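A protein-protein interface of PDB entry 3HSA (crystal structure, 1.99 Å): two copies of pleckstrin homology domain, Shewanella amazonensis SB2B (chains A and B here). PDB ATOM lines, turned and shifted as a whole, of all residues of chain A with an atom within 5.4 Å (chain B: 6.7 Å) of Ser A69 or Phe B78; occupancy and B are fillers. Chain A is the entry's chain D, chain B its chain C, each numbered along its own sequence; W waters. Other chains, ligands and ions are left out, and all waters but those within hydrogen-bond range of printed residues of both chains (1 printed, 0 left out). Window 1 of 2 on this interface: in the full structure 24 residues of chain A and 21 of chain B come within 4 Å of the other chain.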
ATOM      1  N   ARG A  51     -11.716  -5.672 -29.144  1.00  0.00           N
ATOM      2  CA  ARG A  51     -10.727  -5.941 -28.123  1.00  0.00           C
ATOM      3  C   ARG A  51      -9.343  -5.429 -28.477  1.00  0.00           C
ATOM      4  O   ARG A  51      -8.990  -5.175 -29.647  1.00  0.00           O
ATOM      5  CB  ARG A  51     -10.642  -7.464 -27.848  1.00  0.00           C
ATOM      6  CG  ARG A  51     -10.648  -8.273 -29.115  1.00  0.00           C
ATOM      7  CD  ARG A  51     -10.251  -9.732 -28.970  1.00  0.00           C
ATOM      8  NE  ARG A  51     -10.671 -10.410 -30.201  1.00  0.00           N
ATOM      9  CZ  ARG A  51     -10.576 -11.708 -30.428  1.00  0.00           C
ATOM     10  NH1 ARG A  51      -9.955 -12.506 -29.561  1.00  0.00           N
ATOM     11  NH2 ARG A  51     -11.090 -12.206 -31.541  1.00  0.00           N
ATOM     12  N   LEU A  52      -8.583  -5.222 -27.430  1.00  0.00           N
ATOM     13  CA  LEU A  52      -7.169  -5.024 -27.546  1.00  0.00           C
ATOM     14  C   LEU A  52      -6.571  -6.429 -27.503  1.00  0.00           C
ATOM     15  O   LEU A  52      -6.849  -7.189 -26.581  1.00  0.00           O
ATOM     16  CB  LEU A  52      -6.656  -4.223 -26.372  1.00  0.00           C
ATOM     17  CG  LEU A  52      -5.134  -4.119 -26.181  1.00  0.00           C
ATOM     18  CD1 LEU A  52      -4.432  -3.486 -27.402  1.00  0.00           C
ATOM     19  CD2 LEU A  52      -4.884  -3.291 -24.927  1.00  0.00           C
ATOM     20  N   ILE A  53      -5.745  -6.758 -28.486  1.00  0.00           N
ATOM     21  CA  ILE A  53      -5.086  -8.014 -28.544  1.00  0.00           C
ATOM     22  C   ILE A  53      -3.599  -7.711 -28.439  1.00  0.00           C
ATOM     23  O   ILE A  53      -3.069  -7.032 -29.287  1.00  0.00           O
ATOM     24  CB  ILE A  53      -5.335  -8.765 -29.886  1.00  0.00           C
ATOM     25  CG1 ILE A  53      -6.819  -9.073 -30.079  1.00  0.00           C
ATOM     26  CG2 ILE A  53      -4.481 -10.060 -29.950  1.00  0.00           C
ATOM     27  CD1 ILE A  53      -7.178  -9.800 -31.362  1.00  0.00           C
ATOM     28  N   LEU A  54      -2.964  -8.190 -27.388  1.00  0.00           N
ATOM     29  CA  LEU A  54      -1.512  -8.138 -27.248  1.00  0.00           C
ATOM     30  C   LEU A  54      -0.872  -9.376 -27.848  1.00  0.00           C
ATOM     31  O   LEU A  54      -1.134 -10.510 -27.394  1.00  0.00           O
ATOM     32  CB  LEU A  54      -1.099  -8.064 -25.789  1.00  0.00           C
ATOM     33  CG  LEU A  54      -1.034  -6.687 -25.152  1.00  0.00           C
ATOM     34  CD1 LEU A  54      -2.200  -5.780 -25.607  1.00  0.00           C
ATOM     35  CD2 LEU A  54      -0.938  -6.796 -23.633  1.00  0.00           C
ATOM     36  N   TYR A  67      -1.391 -14.659 -27.670  1.00  0.00           N
ATOM     37  CA  TYR A  67      -2.380 -13.673 -28.036  1.00  0.00           C
ATOM     38  C   TYR A  67      -3.179 -13.412 -26.779  1.00  0.00           C
ATOM     39  O   TYR A  67      -3.903 -14.282 -26.336  1.00  0.00           O
ATOM     40  CB  TYR A  67      -3.342 -14.153 -29.138  1.00  0.00           C
ATOM     41  CG  TYR A  67      -2.706 -14.494 -30.454  1.00  0.00           C
ATOM     42  CD1 TYR A  67      -1.686 -13.727 -30.977  1.00  0.00           C
ATOM     43  CD2 TYR A  67      -3.174 -15.553 -31.220  1.00  0.00           C
ATOM     44  CE1 TYR A  67      -1.113 -14.015 -32.209  1.00  0.00           C
ATOM     45  CE2 TYR A  67      -2.589 -15.860 -32.476  1.00  0.00           C
ATOM     46  CZ  TYR A  67      -1.540 -15.088 -32.939  1.00  0.00           C
ATOM     47  OH  TYR A  67      -0.941 -15.353 -34.159  1.00  0.00           O
ATOM     48  N   HIS A  68      -3.042 -12.216 -26.214  1.00  0.00           N
ATOM     49  CA  HIS A  68      -3.787 -11.852 -25.030  1.00  0.00           C
ATOM     50  C   HIS A  68      -4.909 -10.888 -25.450  1.00  0.00           C
ATOM     51  O   HIS A  68      -4.656  -9.732 -25.789  1.00  0.00           O
ATOM     52  CB  HIS A  68      -2.876 -11.197 -24.010  1.00  0.00           C
ATOM     53  CG  HIS A  68      -3.520 -10.976 -22.671  1.00  0.00           C
ATOM     54  ND1 HIS A  68      -2.826 -10.483 -21.584  1.00  0.00           N
ATOM     55  CD2 HIS A  68      -4.783 -11.183 -22.245  1.00  0.00           C
ATOM     56  CE1 HIS A  68      -3.647 -10.405 -20.547  1.00  0.00           C
ATOM     57  NE2 HIS A  68      -4.840 -10.809 -20.929  1.00  0.00           N
ATOM     58  N   SER A  69      -6.139 -11.363 -25.344  1.00  0.00           N
ATOM     59  CA  SER A  69      -7.345 -10.592 -25.714  1.00  0.00           C
ATOM     60  C   SER A  69      -7.930  -9.882 -24.509  1.00  0.00           C
ATOM     61  O   SER A  69      -8.220 -10.509 -23.481  1.00  0.00           O
ATOM     62  CB  SER A  69      -8.388 -11.524 -26.331  1.00  0.00           C
ATOM     63  OG  SER A  69      -7.908 -12.036 -27.561  1.00  0.00           O
ATOM     64  N   ILE A  70      -8.071  -8.561 -24.616  1.00  0.00           N
ATOM     65  CA  ILE A  70      -8.596  -7.748 -23.544  1.00  0.00           C
ATOM     66  C   ILE A  70      -9.791  -6.957 -24.071  1.00  0.00           C
ATOM     67  O   ILE A  70      -9.594  -5.927 -24.781  1.00  0.00           O
ATOM     68  CB  ILE A  70      -7.510  -6.791 -23.003  1.00  0.00           C
ATOM     69  CG1 ILE A  70      -6.262  -7.598 -22.571  1.00  0.00           C
ATOM     70  CG2 ILE A  70      -8.097  -5.919 -21.867  1.00  0.00           C
ATOM     71  CD1 ILE A  70      -5.061  -6.751 -22.239  1.00  0.00           C
ATOM     72  N   PRO A  71     -11.029  -7.439 -23.783  1.00  0.00           N
ATOM     73  CA  PRO A  71     -12.216  -6.673 -24.139  1.00  0.00           C
ATOM     74  C   PRO A  71     -12.079  -5.291 -23.543  1.00  0.00           C
ATOM     75  O   PRO A  71     -11.581  -5.182 -22.425  1.00  0.00           O
ATOM     76  CB  PRO A  71     -13.355  -7.448 -23.466  1.00  0.00           C
ATOM     77  CG  PRO A  71     -12.867  -8.830 -23.345  1.00  0.00           C
ATOM     78  CD  PRO A  71     -11.391  -8.748 -23.180  1.00  0.00           C
ATOM     79  N   ILE B  75     -16.265 -13.686 -17.951  1.00  0.00           N
ATOM     80  CA  ILE B  75     -14.991 -13.891 -18.640  1.00  0.00           C
ATOM     81  C   ILE B  75     -14.453 -12.511 -18.994  1.00  0.00           C
ATOM     82  O   ILE B  75     -14.883 -11.905 -19.966  1.00  0.00           O
ATOM     83  CB  ILE B  75     -15.112 -14.715 -19.898  1.00  0.00           C
ATOM     84  CG1 ILE B  75     -15.665 -16.124 -19.582  1.00  0.00           C
ATOM     85  CG2 ILE B  75     -13.736 -14.823 -20.629  1.00  0.00           C
ATOM     86  CD1 ILE B  75     -16.000 -16.925 -20.844  1.00  0.00           C
ATOM     87  N   VAL B  76     -13.502 -12.011 -18.228  1.00  0.00           N
ATOM     88  CA  VAL B  76     -13.080 -10.622 -18.436  1.00  0.00           C
ATOM     89  C   VAL B  76     -11.935 -10.429 -19.427  1.00  0.00           C
ATOM     90  O   VAL B  76     -11.873  -9.426 -20.039  1.00  0.00           O
ATOM     91  CB  VAL B  76     -12.823  -9.901 -17.140  1.00  0.00           C
ATOM     92  CG1 VAL B  76     -14.190  -9.674 -16.422  1.00  0.00           C
ATOM     93  CG2 VAL B  76     -11.862 -10.681 -16.288  1.00  0.00           C
ATOM     94  N   HIS B  77     -10.989 -11.346 -19.493  1.00  0.00           N
ATOM     95  CA  HIS B  77     -10.024 -11.377 -20.597  1.00  0.00           C
ATOM     96  C   HIS B  77      -9.481 -12.798 -20.686  1.00  0.00           C
ATOM     97  O   HIS B  77      -9.743 -13.622 -19.801  1.00  0.00           O
ATOM     98  CB  HIS B  77      -8.925 -10.304 -20.499  1.00  0.00           C
ATOM     99  CG  HIS B  77      -8.159 -10.293 -19.226  1.00  0.00           C
ATOM    100  ND1 HIS B  77      -6.822 -10.606 -19.163  1.00  0.00           N
ATOM    101  CD2 HIS B  77      -8.517  -9.932 -17.978  1.00  0.00           C
ATOM    102  CE1 HIS B  77      -6.396 -10.481 -17.924  1.00  0.00           C
ATOM    103  NE2 HIS B  77      -7.416 -10.105 -17.177  1.00  0.00           N
ATOM    104  N   PHE B  78      -8.800 -13.097 -21.779  1.00  0.00           N
ATOM    105  CA  PHE B  78      -8.345 -14.447 -22.024  1.00  0.00           C
ATOM    106  C   PHE B  78      -7.116 -14.453 -22.939  1.00  0.00           C
ATOM    107  O   PHE B  78      -6.855 -13.480 -23.651  1.00  0.00           O
ATOM    108  CB  PHE B  78      -9.466 -15.285 -22.617  1.00  0.00           C
ATOM    109  CG  PHE B  78     -10.063 -14.717 -23.884  1.00  0.00           C
ATOM    110  CD1 PHE B  78     -11.104 -13.778 -23.830  1.00  0.00           C
ATOM    111  CD2 PHE B  78      -9.604 -15.136 -25.138  1.00  0.00           C
ATOM    112  CE1 PHE B  78     -11.674 -13.232 -25.020  1.00  0.00           C
ATOM    113  CE2 PHE B  78     -10.179 -14.605 -26.331  1.00  0.00           C
ATOM    114  CZ  PHE B  78     -11.214 -13.663 -26.264  1.00  0.00           C
ATOM    115  N   GLN B  79      -6.380 -15.553 -22.899  1.00  0.00           N
ATOM    116  CA  GLN B  79      -5.138 -15.664 -23.651  1.00  0.00           C
ATOM    117  C   GLN B  79      -4.899 -17.082 -24.098  1.00  0.00           C
ATOM    118  O   GLN B  79      -5.256 -18.010 -23.393  1.00  0.00           O
ATOM    119  CB  GLN B  79      -3.965 -15.241 -22.771  1.00  0.00           C
ATOM    120  CG  GLN B  79      -2.616 -15.509 -23.385  1.00  0.00           C
ATOM    121  CD  GLN B  79      -1.512 -15.065 -22.510  1.00  0.00           C
ATOM    122  OE1 GLN B  79      -1.353 -13.895 -22.290  1.00  0.00           O
ATOM    123  NE2 GLN B  79      -0.733 -15.996 -22.015  1.00  0.00           N
ATOM    124  N   VAL B  80      -4.322 -17.228 -25.289  1.00  0.00           N
ATOM    125  CA  VAL B  80      -3.865 -18.514 -25.755  1.00  0.00           C
ATOM    126  C   VAL B  80      -2.391 -18.319 -26.085  1.00  0.00           C
ATOM    127  O   VAL B  80      -2.019 -17.341 -26.748  1.00  0.00           O
ATOM    128  CB  VAL B  80      -4.665 -19.027 -26.961  1.00  0.00           C
ATOM    129  CG1 VAL B  80      -4.125 -20.378 -27.420  1.00  0.00           C
ATOM    130  CG2 VAL B  80      -6.145 -19.182 -26.577  1.00  0.00           C
ATOM    131  N   LEU B  92      -4.485 -22.227 -22.581  1.00  0.00           N
ATOM    132  CA  LEU B  92      -5.548 -21.215 -22.481  1.00  0.00           C
ATOM    133  C   LEU B  92      -5.607 -20.650 -21.088  1.00  0.00           C
ATOM    134  O   LEU B  92      -5.571 -21.405 -20.100  1.00  0.00           O
ATOM    135  CB  LEU B  92      -6.918 -21.843 -22.805  1.00  0.00           C
ATOM    136  CG  LEU B  92      -8.170 -21.023 -22.513  1.00  0.00           C
ATOM    137  CD1 LEU B  92      -8.354 -19.932 -23.584  1.00  0.00           C
ATOM    138  CD2 LEU B  92      -9.421 -21.950 -22.400  1.00  0.00           C
ATOM    139  N   MLY B  93      -5.695 -19.326 -21.001  1.00  0.00           N
ATOM    140  CA  MLY B  93      -5.899 -18.653 -19.734  1.00  0.00           C
ATOM    141  CB  MLY B  93      -4.740 -17.727 -19.413  1.00  0.00           C
ATOM    142  CG  MLY B  93      -3.524 -18.458 -18.901  1.00  0.00           C
ATOM    143  CD  MLY B  93      -2.359 -17.533 -18.726  1.00  0.00           C
ATOM    144  CE  MLY B  93      -1.146 -18.281 -18.270  1.00  0.00           C
ATOM    145  NZ  MLY B  93       0.139 -17.593 -18.558  1.00  0.00           N
ATOM    146  CH1 MLY B  93       0.201 -16.296 -17.863  1.00  0.00           C
ATOM    147  CH2 MLY B  93       1.233 -18.477 -18.109  1.00  0.00           C
ATOM    148  C   MLY B  93      -7.200 -17.871 -19.815  1.00  0.00           C
ATOM    149  O   MLY B  93      -7.433 -17.154 -20.796  1.00  0.00           O
ATOM    150  N   LEU B  94      -8.069 -18.084 -18.829  1.00  0.00           N
ATOM    151  CA  LEU B  94      -9.337 -17.386 -18.718  1.00  0.00           C
ATOM    152  C   LEU B  94      -9.294 -16.623 -17.408  1.00  0.00           C
ATOM    153  O   LEU B  94      -9.202 -17.226 -16.338  1.00  0.00           O
ATOM    154  CB  LEU B  94     -10.504 -18.367 -18.674  1.00  0.00           C
ATOM    155  CG  LEU B  94     -10.930 -19.127 -19.915  1.00  0.00           C
ATOM    156  CD1 LEU B  94     -12.159 -20.005 -19.519  1.00  0.00           C
ATOM    157  CD2 LEU B  94     -11.283 -18.221 -21.120  1.00  0.00           C
ATOM    158  N   TRP B  95      -9.265 -15.313 -17.482  1.00  0.00           N
ATOM    159  CA  TRP B  95      -9.324 -14.506 -16.282  1.00  0.00           C
ATOM    160  C   TRP B  95     -10.813 -14.232 -16.030  1.00  0.00           C
ATOM    161  O   TRP B  95     -11.557 -13.887 -16.957  1.00  0.00           O
ATOM    162  CB  TRP B  95      -8.523 -13.232 -16.409  1.00  0.00           C
ATOM    163  CG  TRP B  95      -6.986 -13.375 -16.382  1.00  0.00           C
ATOM    164  CD1 TRP B  95      -6.157 -13.258 -15.281  1.00  0.00           C
ATOM    165  CD2 TRP B  95      -6.115 -13.597 -17.505  1.00  0.00           C
ATOM    166  NE1 TRP B  95      -4.825 -13.379 -15.660  1.00  0.00           N
ATOM    167  CE2 TRP B  95      -4.769 -13.589 -17.011  1.00  0.00           C
ATOM    168  CE3 TRP B  95      -6.326 -13.777 -18.872  1.00  0.00           C
ATOM    169  CZ2 TRP B  95      -3.661 -13.789 -17.843  1.00  0.00           C
ATOM    170  CZ3 TRP B  95      -5.216 -13.969 -19.699  1.00  0.00           C
ATOM    171  CH2 TRP B  95      -3.899 -13.974 -19.177  1.00  0.00           C
ATOM    172  N   GLN B 117     -10.894 -20.769 -29.322  1.00  0.00           N
ATOM    173  CA  GLN B 117     -10.564 -19.343 -29.293  1.00  0.00           C
ATOM    174  C   GLN B 117     -11.624 -18.509 -29.987  1.00  0.00           C
ATOM    175  O   GLN B 117     -12.017 -17.472 -29.487  1.00  0.00           O
ATOM    176  CB  GLN B 117      -9.232 -19.060 -30.028  1.00  0.00           C
ATOM    177  CG  GLN B 117      -8.056 -19.482 -29.286  1.00  0.00           C
ATOM    178  CD  GLN B 117      -6.753 -19.259 -30.060  1.00  0.00           C
ATOM    179  OE1 GLN B 117      -6.179 -20.193 -30.619  1.00  0.00           O
ATOM    180  NE2 GLN B 117      -6.299 -18.021 -30.098  1.00  0.00           N
ATOM    181  N   ILE B 120     -14.913 -18.583 -27.834  1.00  0.00           N
ATOM    182  CA  ILE B 120     -14.784 -17.675 -26.690  1.00  0.00           C
ATOM    183  C   ILE B 120     -14.934 -16.205 -27.156  1.00  0.00           C
ATOM    184  O   ILE B 120     -15.649 -15.426 -26.512  1.00  0.00           O
ATOM    185  CB  ILE B 120     -13.445 -17.871 -25.941  1.00  0.00           C
ATOM    186  CG1 ILE B 120     -13.407 -19.222 -25.230  1.00  0.00           C
ATOM    187  CG2 ILE B 120     -13.208 -16.739 -24.934  1.00  0.00           C
ATOM    188  CD1 ILE B 120     -11.960 -19.638 -24.859  1.00  0.00           C
ATOM    189  N   ALA B 121     -14.305 -15.844 -28.285  1.00  0.00           N
ATOM    190  CA  ALA B 121     -14.438 -14.475 -28.837  1.00  0.00           C
ATOM    191  C   ALA B 121     -15.893 -14.116 -29.130  1.00  0.00           C
ATOM    192  O   ALA B 121     -16.345 -13.002 -28.841  1.00  0.00           O
ATOM    193  CB  ALA B 121     -13.601 -14.290 -30.092  1.00  0.00           C
ATOM    194  N   ARG B 122     -16.628 -15.057 -29.680  1.00  0.00           N
ATOM    195  CA  ARG B 122     -17.999 -14.823 -30.042  1.00  0.00           C
ATOM    196  C   ARG B 122     -18.899 -14.633 -28.826  1.00  0.00           C
ATOM    197  O   ARG B 122     -19.843 -13.857 -28.880  1.00  0.00           O
ATOM    198  CB  ARG B 122     -18.519 -15.966 -30.927  1.00  0.00           C
ATOM    199  CG  ARG B 122     -17.837 -15.977 -32.311  1.00  0.00           C
ATOM    200  CD  ARG B 122     -17.747 -17.368 -32.923  1.00  0.00           C
ATOM    201  NE  ARG B 122     -19.023 -18.065 -32.926  1.00  0.00           N
ATOM    202  CZ  ARG B 122     -19.174 -19.385 -32.770  1.00  0.00           C
ATOM    203  NH1 ARG B 122     -18.122 -20.203 -32.596  1.00  0.00           N
ATOM    204  NH2 ARG B 122     -20.404 -19.901 -32.769  1.00  0.00           N
ATOM    205  N   ALA B 124     -17.735 -13.869 -25.513  1.00  0.00           N
ATOM    206  CA  ALA B 124     -17.187 -13.004 -24.490  1.00  0.00           C
ATOM    207  C   ALA B 124     -16.935 -11.602 -24.948  1.00  0.00           C
ATOM    208  O   ALA B 124     -16.499 -10.800 -24.137  1.00  0.00           O
ATOM    209  CB  ALA B 124     -15.891 -13.609 -23.934  1.00  0.00           C
ATOM    210  N   LEU B 125     -17.192 -11.253 -26.202  1.00  0.00           N
ATOM    211  CA  LEU B 125     -16.803  -9.903 -26.665  1.00  0.00           C
ATOM    212  C   LEU B 125     -17.968  -8.929 -26.796  1.00  0.00           C
ATOM    213  O   LEU B 125     -17.792  -7.749 -26.486  1.00  0.00           O
ATOM    214  CB  LEU B 125     -15.969  -9.945 -27.958  1.00  0.00           C
ATOM    215  CG  LEU B 125     -14.581 -10.572 -27.818  1.00  0.00           C
ATOM    216  CD1 LEU B 125     -13.819 -10.535 -29.099  1.00  0.00           C
ATOM    217  CD2 LEU B 125     -13.761  -9.888 -26.712  1.00  0.00           C
HETATM  218  O   HOH W   1     -10.163 -15.386 -30.198  1.00  0.00           O
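Of the 9 printed residues of chain A, 6 touch a printed residue of chain B.
Hydrophobic or aromatic side chains of chain A within 4 Å of the printed part of chain B: His A68 and Pro A71.
Of the 16 printed residues of chain B, 8 touch a printed residue of chain A.
Hydrophobic or aromatic side chains of chain B that line the printed part of chain A: His B77, Phe B78, Trp B95, Ala B121 and Leu B125.
Among the printed residues, no Asp or Glu carboxylate lies within 4 Å of a Lys or Arg side-chain nitrogen of the other chain.
Ile A53 touches none of the printed residues of chain B.
Of the printed residues of chain B, Ile A70 touches His B77.
Printed residues of chain A within 4 Å of Val B76: Pro A71 (3.2 Å).
Of chain A, only Arg A51, His A68 and Ser A69 come within 4 Å of Phe B78.
Of the printed residues of chain A, Gln B79 touches Tyr A67 and His A68.
Printed residues of chain A within 4 Å of Val B80: Tyr A67 (2.9 Å).
Of the printed residues of chain A, Trp B95 touches His A68.
Gln B117 touches none of the printed residues of chain A.
Water W1 lies within hydrogen-bond range of O of Gln B117 and NH1 of Arg A51.
No position is printed for both chains.
Of the 15 pairs that touch across the chains among the printed residues, none has its exchanged pair printed and touching as well.
ND1 of His B77 is in hydrogen-bond range of NE2 of His A68, at 2.7 Å.
N of Ser A69 is in hydrogen-bond range of O of Phe B78 (2.8 Å).
O of Val B80 lies within hydrogen-bond range of N of Tyr A67 (2.9 Å).
Among the printed residues, pairs that only touch across the chains: Arg A51 with Phe B78, Arg A51 with Ala B121, Arg A51 with Leu B125, Tyr A67 with Gln B79, His A68 with Phe B78, His A68 with Gln B79, His A68 with Trp B95, Ser A69 with His B77, Ile A70 with His B77, Pro A71 with Val B76, Pro A71 with His B77 and Pro A71 with Leu B125.
O of Trp B95 sits at hydrogen-bond distance from N of Val B76, at 3.0 Å.
O of His B77 sits at hydrogen-bond distance from N of Trp B95.
The backbone carbonyl oxygen (O) of Gln B79 sits at hydrogen-bond distance from N of MLY B93, at 2.8 Å.
OG of Ser A69 sits at hydrogen-bond distance from NH1 of Arg A51.
The backbone NH (N) of Ile A70 sits at hydrogen-bond distance from the backbone carbonyl oxygen (O) of Leu A52, 2.7 Å away.
The backbone carbonyl oxygen of His A68 sits at hydrogen-bond distance from the backbone NH of Leu A54.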
